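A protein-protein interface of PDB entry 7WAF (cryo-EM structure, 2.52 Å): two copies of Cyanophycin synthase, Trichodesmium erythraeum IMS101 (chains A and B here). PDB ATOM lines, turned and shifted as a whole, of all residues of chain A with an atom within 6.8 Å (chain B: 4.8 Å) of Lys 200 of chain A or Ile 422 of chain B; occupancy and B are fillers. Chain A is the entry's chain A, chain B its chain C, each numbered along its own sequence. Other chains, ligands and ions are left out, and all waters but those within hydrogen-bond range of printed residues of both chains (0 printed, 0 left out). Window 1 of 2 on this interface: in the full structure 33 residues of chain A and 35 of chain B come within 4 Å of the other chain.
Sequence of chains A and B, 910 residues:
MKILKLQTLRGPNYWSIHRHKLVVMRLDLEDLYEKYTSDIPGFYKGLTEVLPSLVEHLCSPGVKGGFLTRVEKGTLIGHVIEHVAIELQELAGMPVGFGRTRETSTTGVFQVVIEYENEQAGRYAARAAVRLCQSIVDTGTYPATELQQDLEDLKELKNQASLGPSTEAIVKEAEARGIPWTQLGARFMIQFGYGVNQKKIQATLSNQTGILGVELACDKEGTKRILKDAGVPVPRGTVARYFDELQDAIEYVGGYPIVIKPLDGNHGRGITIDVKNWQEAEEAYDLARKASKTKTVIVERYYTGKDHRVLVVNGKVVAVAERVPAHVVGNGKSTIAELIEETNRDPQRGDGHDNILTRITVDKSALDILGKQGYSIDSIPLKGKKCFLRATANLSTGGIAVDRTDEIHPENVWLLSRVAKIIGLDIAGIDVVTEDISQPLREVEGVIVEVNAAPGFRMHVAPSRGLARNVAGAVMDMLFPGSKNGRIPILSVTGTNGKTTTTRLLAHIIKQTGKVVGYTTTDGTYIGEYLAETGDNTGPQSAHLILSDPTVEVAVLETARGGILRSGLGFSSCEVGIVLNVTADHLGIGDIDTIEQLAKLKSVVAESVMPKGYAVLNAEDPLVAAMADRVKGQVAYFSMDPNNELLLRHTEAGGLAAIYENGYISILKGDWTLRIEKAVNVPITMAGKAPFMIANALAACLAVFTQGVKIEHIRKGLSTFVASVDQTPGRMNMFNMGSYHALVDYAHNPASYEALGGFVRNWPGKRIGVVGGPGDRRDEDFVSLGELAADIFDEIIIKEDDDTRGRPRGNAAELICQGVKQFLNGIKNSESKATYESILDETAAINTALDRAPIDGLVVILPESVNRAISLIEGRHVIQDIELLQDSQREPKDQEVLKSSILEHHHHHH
The side-chain amino group of Lys 200 of chain A sits at hydrogen-bond distance from the backbone carbonyl oxygen of Ile 422 of chain B (3.3 Å). NE of Arg 418 of chain B is in salt-bridge range of OD1 of Asp 549 of chain A (3.7 Å).
N of Leu 184 of chain A is in hydrogen-bond range of O of Met 189 of chain A (2.8 Å). OG of Ser 206 of chain A lies close to N of Gln 208 of chain A (3.4 Å). O of Ala 230 of chain B is in hydrogen-bond range of NH2 of Arg 418 of chain B (2.8 Å). The backbone NH (N) of Asn 207 of chain A lies within hydrogen-bond range of the backbone carbonyl oxygen (O) of Lys 200 of chain A, at 2.8 Å.
CD1 of Leu 212 of chain B touches SD of Met 189 of chain A, 3.8 Å away. Lys 200 of chain A touches Leu 212 of chain B (O to CD1, 3.9 Å). Gln 202 of chain A touches Leu 212 of chain B. C of Ser 206 of chain A touches CD1 of Leu 212 of chain B (3.8 Å). Asn 207 of chain A touches Leu 212 of chain B. Pro 550 of chain A touches Lys 421 of chain B (CG to CB, 3.7 Å). Pro 550 of chain A touches Ile 422 of chain B (CD to CG1, 3.7 Å).
Lys 200 of chain A touches just these residues of chain B: Leu 212 and Ile 422. Ile 422 of chain B touches two residues of chain A. Of the printed residues of chain B, Ser 206 of chain A touches Leu 212 (3.8 Å). Printed residues of chain A within 4 Å of Leu 212 of chain B: Met 189, Lys 200, Gln 202, Ser 206 and Asn 207. Gln 191 of chain A touches none of the printed residues of chain B.
Of the 12 printed residues of chain B, 4 touch a printed residue of chain A. Hydrophobic or aromatic side chains of chain B that line the printed part of chain A: Leu 212 and Ile 422. Hydrophobic or aromatic side chains of chain A that line the printed part of chain B: Met 189 and Pro 550. Among the printed residues, 9 pairs touch across the chains.
No position is printed for both chains.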
ATOM      1  N   LEU A 184     -26.161 -12.598  -2.461  1.00  0.00           N
ATOM      2  CA  LEU A 184     -25.118 -11.589  -2.354  1.00  0.00           C
ATOM      3  C   LEU A 184     -24.895 -11.221  -0.892  1.00  0.00           C
ATOM      4  O   LEU A 184     -25.793 -11.336  -0.053  1.00  0.00           O
ATOM      5  CB  LEU A 184     -25.490 -10.348  -3.164  1.00  0.00           C
ATOM      6  CG  LEU A 184     -25.751 -10.581  -4.652  1.00  0.00           C
ATOM      7  CD1 LEU A 184     -25.884  -9.260  -5.385  1.00  0.00           C
ATOM      8  CD2 LEU A 184     -24.648 -11.424  -5.265  1.00  0.00           C
ATOM      9  N   MET A 189     -29.478  -9.249  -0.929  1.00  0.00           N
ATOM     10  CA  MET A 189     -29.847  -9.282  -2.334  1.00  0.00           C
ATOM     11  C   MET A 189     -29.600 -10.666  -2.913  1.00  0.00           C
ATOM     12  O   MET A 189     -28.591 -11.311  -2.612  1.00  0.00           O
ATOM     13  CB  MET A 189     -29.064  -8.236  -3.129  1.00  0.00           C
ATOM     14  CG  MET A 189     -29.262  -6.813  -2.645  1.00  0.00           C
ATOM     15  SD  MET A 189     -29.223  -5.616  -3.992  1.00  0.00           S
ATOM     16  CE  MET A 189     -27.465  -5.314  -4.122  1.00  0.00           C
ATOM     17  N   ILE A 190     -30.533 -11.118  -3.743  1.00  0.00           N
ATOM     18  CA  ILE A 190     -30.449 -12.397  -4.431  1.00  0.00           C
ATOM     19  C   ILE A 190     -30.196 -12.127  -5.903  1.00  0.00           C
ATOM     20  O   ILE A 190     -30.905 -11.324  -6.528  1.00  0.00           O
ATOM     21  CB  ILE A 190     -31.727 -13.229  -4.236  1.00  0.00           C
ATOM     22  CG1 ILE A 190     -31.995 -13.453  -2.748  1.00  0.00           C
ATOM     23  CG2 ILE A 190     -31.617 -14.552  -4.970  1.00  0.00           C
ATOM     24  CD1 ILE A 190     -30.988 -14.354  -2.079  1.00  0.00           C
ATOM     25  N   GLN A 191     -29.183 -12.788  -6.455  1.00  0.00           N
ATOM     26  CA  GLN A 191     -28.835 -12.679  -7.863  1.00  0.00           C
ATOM     27  C   GLN A 191     -29.291 -13.929  -8.603  1.00  0.00           C
ATOM     28  O   GLN A 191     -28.933 -15.046  -8.220  1.00  0.00           O
ATOM     29  CB  GLN A 191     -27.331 -12.486  -8.043  1.00  0.00           C
ATOM     30  CG  GLN A 191     -26.882 -12.514  -9.492  1.00  0.00           C
ATOM     31  CD  GLN A 191     -25.422 -12.877  -9.645  1.00  0.00           C
ATOM     32  OE1 GLN A 191     -24.562 -12.347  -8.944  1.00  0.00           O
ATOM     33  NE2 GLN A 191     -25.133 -13.785 -10.567  1.00  0.00           N
ATOM     34  N   PHE A 192     -30.071 -13.733  -9.658  1.00  0.00           N
ATOM     35  CA  PHE A 192     -30.530 -14.811 -10.519  1.00  0.00           C
ATOM     36  C   PHE A 192     -29.747 -14.789 -11.824  1.00  0.00           C
ATOM     37  O   PHE A 192     -29.471 -13.721 -12.376  1.00  0.00           O
ATOM     38  CB  PHE A 192     -32.025 -14.679 -10.813  1.00  0.00           C
ATOM     39  CG  PHE A 192     -32.890 -14.729  -9.591  1.00  0.00           C
ATOM     40  CD1 PHE A 192     -33.042 -15.905  -8.883  1.00  0.00           C
ATOM     41  CD2 PHE A 192     -33.556 -13.600  -9.153  1.00  0.00           C
ATOM     42  CE1 PHE A 192     -33.839 -15.953  -7.759  1.00  0.00           C
ATOM     43  CE2 PHE A 192     -34.355 -13.644  -8.031  1.00  0.00           C
ATOM     44  CZ  PHE A 192     -34.496 -14.821  -7.333  1.00  0.00           C
ATOM     45  N   GLN A 198     -27.943 -11.759 -15.835  1.00  0.00           N
ATOM     46  CA  GLN A 198     -28.317 -11.803 -14.431  1.00  0.00           C
ATOM     47  C   GLN A 198     -29.326 -10.714 -14.084  1.00  0.00           C
ATOM     48  O   GLN A 198     -29.396  -9.668 -14.732  1.00  0.00           O
ATOM     49  CB  GLN A 198     -27.081 -11.657 -13.543  1.00  0.00           C
ATOM     50  CG  GLN A 198     -26.495 -10.259 -13.528  1.00  0.00           C
ATOM     51  CD  GLN A 198     -25.287 -10.145 -12.627  1.00  0.00           C
ATOM     52  OE1 GLN A 198     -25.394  -9.724 -11.479  1.00  0.00           O
ATOM     53  NE2 GLN A 198     -24.126 -10.520 -13.147  1.00  0.00           N
ATOM     54  N   LYS A 199     -30.115 -10.986 -13.047  1.00  0.00           N
ATOM     55  CA  LYS A 199     -31.017 -10.017 -12.442  1.00  0.00           C
ATOM     56  C   LYS A 199     -30.801 -10.042 -10.936  1.00  0.00           C
ATOM     57  O   LYS A 199     -30.192 -10.964 -10.396  1.00  0.00           O
ATOM     58  CB  LYS A 199     -32.485 -10.321 -12.768  1.00  0.00           C
ATOM     59  CG  LYS A 199     -32.775 -10.498 -14.244  1.00  0.00           C
ATOM     60  CD  LYS A 199     -32.797  -9.166 -14.962  1.00  0.00           C
ATOM     61  CE  LYS A 199     -32.907  -9.352 -16.462  1.00  0.00           C
ATOM     62  NZ  LYS A 199     -32.814  -8.055 -17.183  1.00  0.00           N
ATOM     63  N   LYS A 200     -31.302  -9.017 -10.254  1.00  0.00           N
ATOM     64  CA  LYS A 200     -31.170  -8.926  -8.806  1.00  0.00           C
ATOM     65  C   LYS A 200     -32.496  -8.526  -8.185  1.00  0.00           C
ATOM     66  O   LYS A 200     -33.231  -7.707  -8.745  1.00  0.00           O
ATOM     67  CB  LYS A 200     -30.090  -7.919  -8.406  1.00  0.00           C
ATOM     68  CG  LYS A 200     -28.672  -8.411  -8.604  1.00  0.00           C
ATOM     69  CD  LYS A 200     -27.671  -7.324  -8.273  1.00  0.00           C
ATOM     70  CE  LYS A 200     -26.404  -7.472  -9.091  1.00  0.00           C
ATOM     71  NZ  LYS A 200     -25.554  -6.255  -9.008  1.00  0.00           N
ATOM     72  N   ILE A 201     -32.802  -9.110  -7.029  1.00  0.00           N
ATOM     73  CA  ILE A 201     -33.960  -8.714  -6.235  1.00  0.00           C
ATOM     74  C   ILE A 201     -33.521  -8.571  -4.786  1.00  0.00           C
ATOM     75  O   ILE A 201     -32.532  -9.171  -4.362  1.00  0.00           O
ATOM     76  CB  ILE A 201     -35.126  -9.722  -6.343  1.00  0.00           C
ATOM     77  CG1 ILE A 201     -34.752 -11.044  -5.672  1.00  0.00           C
ATOM     78  CG2 ILE A 201     -35.523  -9.942  -7.791  1.00  0.00           C
ATOM     79  CD1 ILE A 201     -35.935 -11.812  -5.139  1.00  0.00           C
ATOM     80  N   GLN A 202     -34.243  -7.750  -4.024  1.00  0.00           N
ATOM     81  CA  GLN A 202     -33.988  -7.741  -2.589  1.00  0.00           C
ATOM     82  C   GLN A 202     -35.055  -8.522  -1.834  1.00  0.00           C
ATOM     83  O   GLN A 202     -34.769  -9.574  -1.253  1.00  0.00           O
ATOM     84  CB  GLN A 202     -33.923  -6.306  -2.067  1.00  0.00           C
ATOM     85  CG  GLN A 202     -33.257  -6.175  -0.714  1.00  0.00           C
ATOM     86  CD  GLN A 202     -33.122  -4.736  -0.272  1.00  0.00           C
ATOM     87  OE1 GLN A 202     -34.094  -3.983  -0.270  1.00  0.00           O
ATOM     88  NE2 GLN A 202     -31.912  -4.344   0.102  1.00  0.00           N
ATOM     89  N   LEU A 205     -38.415  -5.483  -4.715  1.00  0.00           N
ATOM     90  CA  LEU A 205     -37.709  -4.606  -5.637  1.00  0.00           C
ATOM     91  C   LEU A 205     -36.753  -5.414  -6.502  1.00  0.00           C
ATOM     92  O   LEU A 205     -35.999  -6.254  -6.005  1.00  0.00           O
ATOM     93  CB  LEU A 205     -36.926  -3.545  -4.867  1.00  0.00           C
ATOM     94  CG  LEU A 205     -37.661  -2.730  -3.807  1.00  0.00           C
ATOM     95  CD1 LEU A 205     -36.667  -2.036  -2.897  1.00  0.00           C
ATOM     96  CD2 LEU A 205     -38.575  -1.718  -4.467  1.00  0.00           C
ATOM     97  N   SER A 206     -36.782  -5.154  -7.800  1.00  0.00           N
ATOM     98  CA  SER A 206     -35.818  -5.724  -8.725  1.00  0.00           C
ATOM     99  C   SER A 206     -34.757  -4.684  -9.062  1.00  0.00           C
ATOM    100  O   SER A 206     -34.856  -3.513  -8.693  1.00  0.00           O
ATOM    101  CB  SER A 206     -36.512  -6.222  -9.995  1.00  0.00           C
ATOM    102  OG  SER A 206     -37.048  -5.147 -10.742  1.00  0.00           O
ATOM    103  N   ASN A 207     -33.723  -5.129  -9.775  1.00  0.00           N
ATOM    104  CA  ASN A 207     -32.681  -4.205 -10.201  1.00  0.00           C
ATOM    105  C   ASN A 207     -33.168  -3.229 -11.263  1.00  0.00           C
ATOM    106  O   ASN A 207     -32.459  -2.263 -11.563  1.00  0.00           O
ATOM    107  CB  ASN A 207     -31.466  -4.978 -10.714  1.00  0.00           C
ATOM    108  CG  ASN A 207     -31.771  -5.786 -11.956  1.00  0.00           C
ATOM    109  OD1 ASN A 207     -32.858  -6.343 -12.097  1.00  0.00           O
ATOM    110  ND2 ASN A 207     -30.809  -5.856 -12.865  1.00  0.00           N
ATOM    111  N   GLN A 208     -34.348  -3.455 -11.835  1.00  0.00           N
ATOM    112  CA  GLN A 208     -34.945  -2.542 -12.798  1.00  0.00           C
ATOM    113  C   GLN A 208     -35.996  -1.631 -12.179  1.00  0.00           C
ATOM    114  O   GLN A 208     -36.609  -0.839 -12.900  1.00  0.00           O
ATOM    115  CB  GLN A 208     -35.562  -3.330 -13.956  1.00  0.00           C
ATOM    116  CG  GLN A 208     -34.578  -4.238 -14.671  1.00  0.00           C
ATOM    117  CD  GLN A 208     -35.215  -5.011 -15.807  1.00  0.00           C
ATOM    118  OE1 GLN A 208     -35.948  -5.974 -15.583  1.00  0.00           O
ATOM    119  NE2 GLN A 208     -34.937  -4.592 -17.035  1.00  0.00           N
ATOM    120  N   LEU A 479     -38.949 -10.983 -14.761  1.00  0.00           N
ATOM    121  CA  LEU A 479     -37.490 -10.988 -14.740  1.00  0.00           C
ATOM    122  C   LEU A 479     -36.913 -11.726 -15.942  1.00  0.00           C
ATOM    123  O   LEU A 479     -35.931 -11.273 -16.542  1.00  0.00           O
ATOM    124  CB  LEU A 479     -36.991 -11.611 -13.437  1.00  0.00           C
ATOM    125  CG  LEU A 479     -37.163 -10.743 -12.192  1.00  0.00           C
ATOM    126  CD1 LEU A 479     -36.689 -11.482 -10.955  1.00  0.00           C
ATOM    127  CD2 LEU A 479     -36.424  -9.429 -12.352  1.00  0.00           C
ATOM    128  N   SER A 548     -20.659 -13.842 -11.532  1.00  0.00           N
ATOM    129  CA  SER A 548     -21.413 -12.689 -11.059  1.00  0.00           C
ATOM    130  C   SER A 548     -21.029 -11.395 -11.760  1.00  0.00           C
ATOM    131  O   SER A 548     -21.616 -10.351 -11.463  1.00  0.00           O
ATOM    132  CB  SER A 548     -21.234 -12.527  -9.547  1.00  0.00           C
ATOM    133  OG  SER A 548     -19.969 -11.971  -9.242  1.00  0.00           O
ATOM    134  N   ASP A 549     -20.070 -11.432 -12.675  1.00  0.00           N
ATOM    135  CA  ASP A 549     -19.660 -10.216 -13.365  1.00  0.00           C
ATOM    136  C   ASP A 549     -20.701  -9.835 -14.408  1.00  0.00           C
ATOM    137  O   ASP A 549     -21.113 -10.685 -15.206  1.00  0.00           O
ATOM    138  CB  ASP A 549     -18.298 -10.398 -14.022  1.00  0.00           C
ATOM    139  CG  ASP A 549     -17.718  -9.092 -14.520  1.00  0.00           C
ATOM    140  OD1 ASP A 549     -17.044  -8.402 -13.728  1.00  0.00           O
ATOM    141  OD2 ASP A 549     -17.936  -8.752 -15.701  1.00  0.00           O
ATOM    142  N   PRO A 550     -21.145  -8.575 -14.448  1.00  0.00           N
ATOM    143  CA  PRO A 550     -22.229  -8.201 -15.369  1.00  0.00           C
ATOM    144  C   PRO A 550     -21.818  -8.139 -16.831  1.00  0.00           C
ATOM    145  O   PRO A 550     -22.692  -7.939 -17.683  1.00  0.00           O
ATOM    146  CB  PRO A 550     -22.654  -6.820 -14.860  1.00  0.00           C
ATOM    147  CG  PRO A 550     -21.427  -6.274 -14.214  1.00  0.00           C
ATOM    148  CD  PRO A 550     -20.722  -7.447 -13.599  1.00  0.00           C
ATOM    149  N   LEU B 212     -31.961  -0.439  -6.145  1.00  0.00           N
ATOM    150  CA  LEU B 212     -30.965  -1.287  -5.498  1.00  0.00           C
ATOM    151  C   LEU B 212     -29.564  -0.710  -5.647  1.00  0.00           C
ATOM    152  O   LEU B 212     -28.792  -0.687  -4.684  1.00  0.00           O
ATOM    153  CB  LEU B 212     -31.033  -2.700  -6.075  1.00  0.00           C
ATOM    154  CG  LEU B 212     -32.334  -3.456  -5.802  1.00  0.00           C
ATOM    155  CD1 LEU B 212     -32.219  -4.901  -6.249  1.00  0.00           C
ATOM    156  CD2 LEU B 212     -32.701  -3.373  -4.333  1.00  0.00           C
ATOM    157  N   ILE B 226     -19.030  -5.682  -1.841  1.00  0.00           N
ATOM    158  CA  ILE B 226     -19.361  -6.114  -3.196  1.00  0.00           C
ATOM    159  C   ILE B 226     -18.175  -5.914  -4.128  1.00  0.00           C
ATOM    160  O   ILE B 226     -17.849  -6.790  -4.938  1.00  0.00           O
ATOM    161  CB  ILE B 226     -20.611  -5.372  -3.704  1.00  0.00           C
ATOM    162  CG1 ILE B 226     -21.853  -5.875  -2.978  1.00  0.00           C
ATOM    163  CG2 ILE B 226     -20.781  -5.573  -5.194  1.00  0.00           C
ATOM    164  CD1 ILE B 226     -22.136  -7.339  -3.198  1.00  0.00           C
ATOM    165  N   LEU B 227     -17.506  -4.763  -4.028  1.00  0.00           N
ATOM    166  CA  LEU B 227     -16.371  -4.499  -4.905  1.00  0.00           C
ATOM    167  C   LEU B 227     -15.206  -5.432  -4.603  1.00  0.00           C
ATOM    168  O   LEU B 227     -14.504  -5.870  -5.519  1.00  0.00           O
ATOM    169  CB  LEU B 227     -15.946  -3.038  -4.781  1.00  0.00           C
ATOM    170  CG  LEU B 227     -16.925  -2.010  -5.347  1.00  0.00           C
ATOM    171  CD1 LEU B 227     -16.297  -0.629  -5.373  1.00  0.00           C
ATOM    172  CD2 LEU B 227     -17.390  -2.417  -6.733  1.00  0.00           C
ATOM    173  N   ALA B 230     -15.577  -8.688  -6.167  1.00  0.00           N
ATOM    174  CA  ALA B 230     -15.382  -8.626  -7.607  1.00  0.00           C
ATOM    175  C   ALA B 230     -13.930  -8.390  -7.998  1.00  0.00           C
ATOM    176  O   ALA B 230     -13.643  -8.186  -9.181  1.00  0.00           O
ATOM    177  CB  ALA B 230     -16.266  -7.535  -8.210  1.00  0.00           C
ATOM    178  N   VAL B 232     -12.086  -5.804  -7.179  1.00  0.00           N
ATOM    179  CA  VAL B 232     -11.781  -4.379  -7.263  1.00  0.00           C
ATOM    180  C   VAL B 232     -10.886  -3.989  -6.091  1.00  0.00           C
ATOM    181  O   VAL B 232     -11.137  -4.412  -4.955  1.00  0.00           O
ATOM    182  CB  VAL B 232     -13.070  -3.544  -7.289  1.00  0.00           C
ATOM    183  CG1 VAL B 232     -12.754  -2.068  -7.431  1.00  0.00           C
ATOM    184  CG2 VAL B 232     -13.970  -4.007  -8.421  1.00  0.00           C
ATOM    185  N   ARG B 418     -16.587  -1.342 -15.220  1.00  0.00           N
ATOM    186  CA  ARG B 418     -17.025  -2.561 -14.551  1.00  0.00           C
ATOM    187  C   ARG B 418     -17.559  -2.263 -13.156  1.00  0.00           C
ATOM    188  O   ARG B 418     -18.542  -2.869 -12.726  1.00  0.00           O
ATOM    189  CB  ARG B 418     -15.876  -3.563 -14.481  1.00  0.00           C
ATOM    190  CG  ARG B 418     -16.327  -5.008 -14.469  1.00  0.00           C
ATOM    191  CD  ARG B 418     -15.159  -5.954 -14.655  1.00  0.00           C
ATOM    192  NE  ARG B 418     -14.248  -5.917 -13.519  1.00  0.00           N
ATOM    193  CZ  ARG B 418     -14.276  -6.774 -12.508  1.00  0.00           C
ATOM    194  NH1 ARG B 418     -15.174  -7.743 -12.448  1.00  0.00           N
ATOM    195  NH2 ARG B 418     -13.382  -6.655 -11.532  1.00  0.00           N
ATOM    196  N   VAL B 419     -16.915  -1.347 -12.433  1.00  0.00           N
ATOM    197  CA  VAL B 419     -17.380  -0.987 -11.094  1.00  0.00           C
ATOM    198  C   VAL B 419     -18.771  -0.371 -11.164  1.00  0.00           C
ATOM    199  O   VAL B 419     -19.666  -0.711 -10.377  1.00  0.00           O
ATOM    200  CB  VAL B 419     -16.376  -0.034 -10.419  1.00  0.00           C
ATOM    201  CG1 VAL B 419     -17.027   0.690  -9.254  1.00  0.00           C
ATOM    202  CG2 VAL B 419     -15.151  -0.796  -9.959  1.00  0.00           C
ATOM    203  N   ALA B 420     -18.973   0.542 -12.117  1.00  0.00           N
ATOM    204  CA  ALA B 420     -20.279   1.172 -12.266  1.00  0.00           C
ATOM    205  C   ALA B 420     -21.350   0.146 -12.615  1.00  0.00           C
ATOM    206  O   ALA B 420     -22.480   0.226 -12.122  1.00  0.00           O
ATOM    207  CB  ALA B 420     -20.218   2.266 -13.330  1.00  0.00           C
ATOM    208  N   LYS B 421     -21.015  -0.824 -13.470  1.00  0.00           N
ATOM    209  CA  LYS B 421     -21.983  -1.868 -13.797  1.00  0.00           C
ATOM    210  C   LYS B 421     -22.242  -2.797 -12.615  1.00  0.00           C
ATOM    211  O   LYS B 421     -23.372  -3.262 -12.432  1.00  0.00           O
ATOM    212  CB  LYS B 421     -21.504  -2.670 -15.005  1.00  0.00           C
ATOM    213  CG  LYS B 421     -21.444  -1.869 -16.290  1.00  0.00           C
ATOM    214  CD  LYS B 421     -21.479  -2.775 -17.504  1.00  0.00           C
ATOM    215  CE  LYS B 421     -21.022  -2.041 -18.752  1.00  0.00           C
ATOM    216  NZ  LYS B 421     -19.540  -2.020 -18.868  1.00  0.00           N
ATOM    217  N   ILE B 422     -21.216  -3.081 -11.812  1.00  0.00           N
ATOM    218  CA  ILE B 422     -21.375  -3.978 -10.671  1.00  0.00           C
ATOM    219  C   ILE B 422     -22.289  -3.352  -9.628  1.00  0.00           C
ATOM    220  O   ILE B 422     -23.187  -4.012  -9.090  1.00  0.00           O
ATOM    221  CB  ILE B 422     -20.002  -4.334 -10.074  1.00  0.00           C
ATOM    222  CG1 ILE B 422     -19.278  -5.351 -10.954  1.00  0.00           C
ATOM    223  CG2 ILE B 422     -20.152  -4.877  -8.668  1.00  0.00           C
ATOM    224  CD1 ILE B 422     -17.784  -5.371 -10.743  1.00  0.00           C
ATOM    225  N   ILE B 423     -22.074  -2.073  -9.320  1.00  0.00           N
ATOM    226  CA  ILE B 423     -22.938  -1.404  -8.353  1.00  0.00           C
ATOM    227  C   ILE B 423     -24.362  -1.309  -8.890  1.00  0.00           C
ATOM    228  O   ILE B 423     -25.333  -1.505  -8.149  1.00  0.00           O
ATOM    229  CB  ILE B 423     -22.368  -0.023  -7.987  1.00  0.00           C
ATOM    230  CG1 ILE B 423     -20.980  -0.174  -7.367  1.00  0.00           C
ATOM    231  CG2 ILE B 423     -23.293   0.696  -7.023  1.00  0.00           C
ATOM    232  CD1 ILE B 423     -20.956  -1.050  -6.137  1.00  0.00           C
ATOM    233  N   GLY B 424     -24.510  -1.023 -10.179  1.00  0.00           N
ATOM    234  CA  GLY B 424     -25.820  -0.979 -10.796  1.00  0.00           C
ATOM    235  C   GLY B 424     -26.345   0.426 -10.991  1.00  0.00           C
ATOM    236  O   GLY B 424     -27.524   0.694 -10.744  1.00  0.00           O
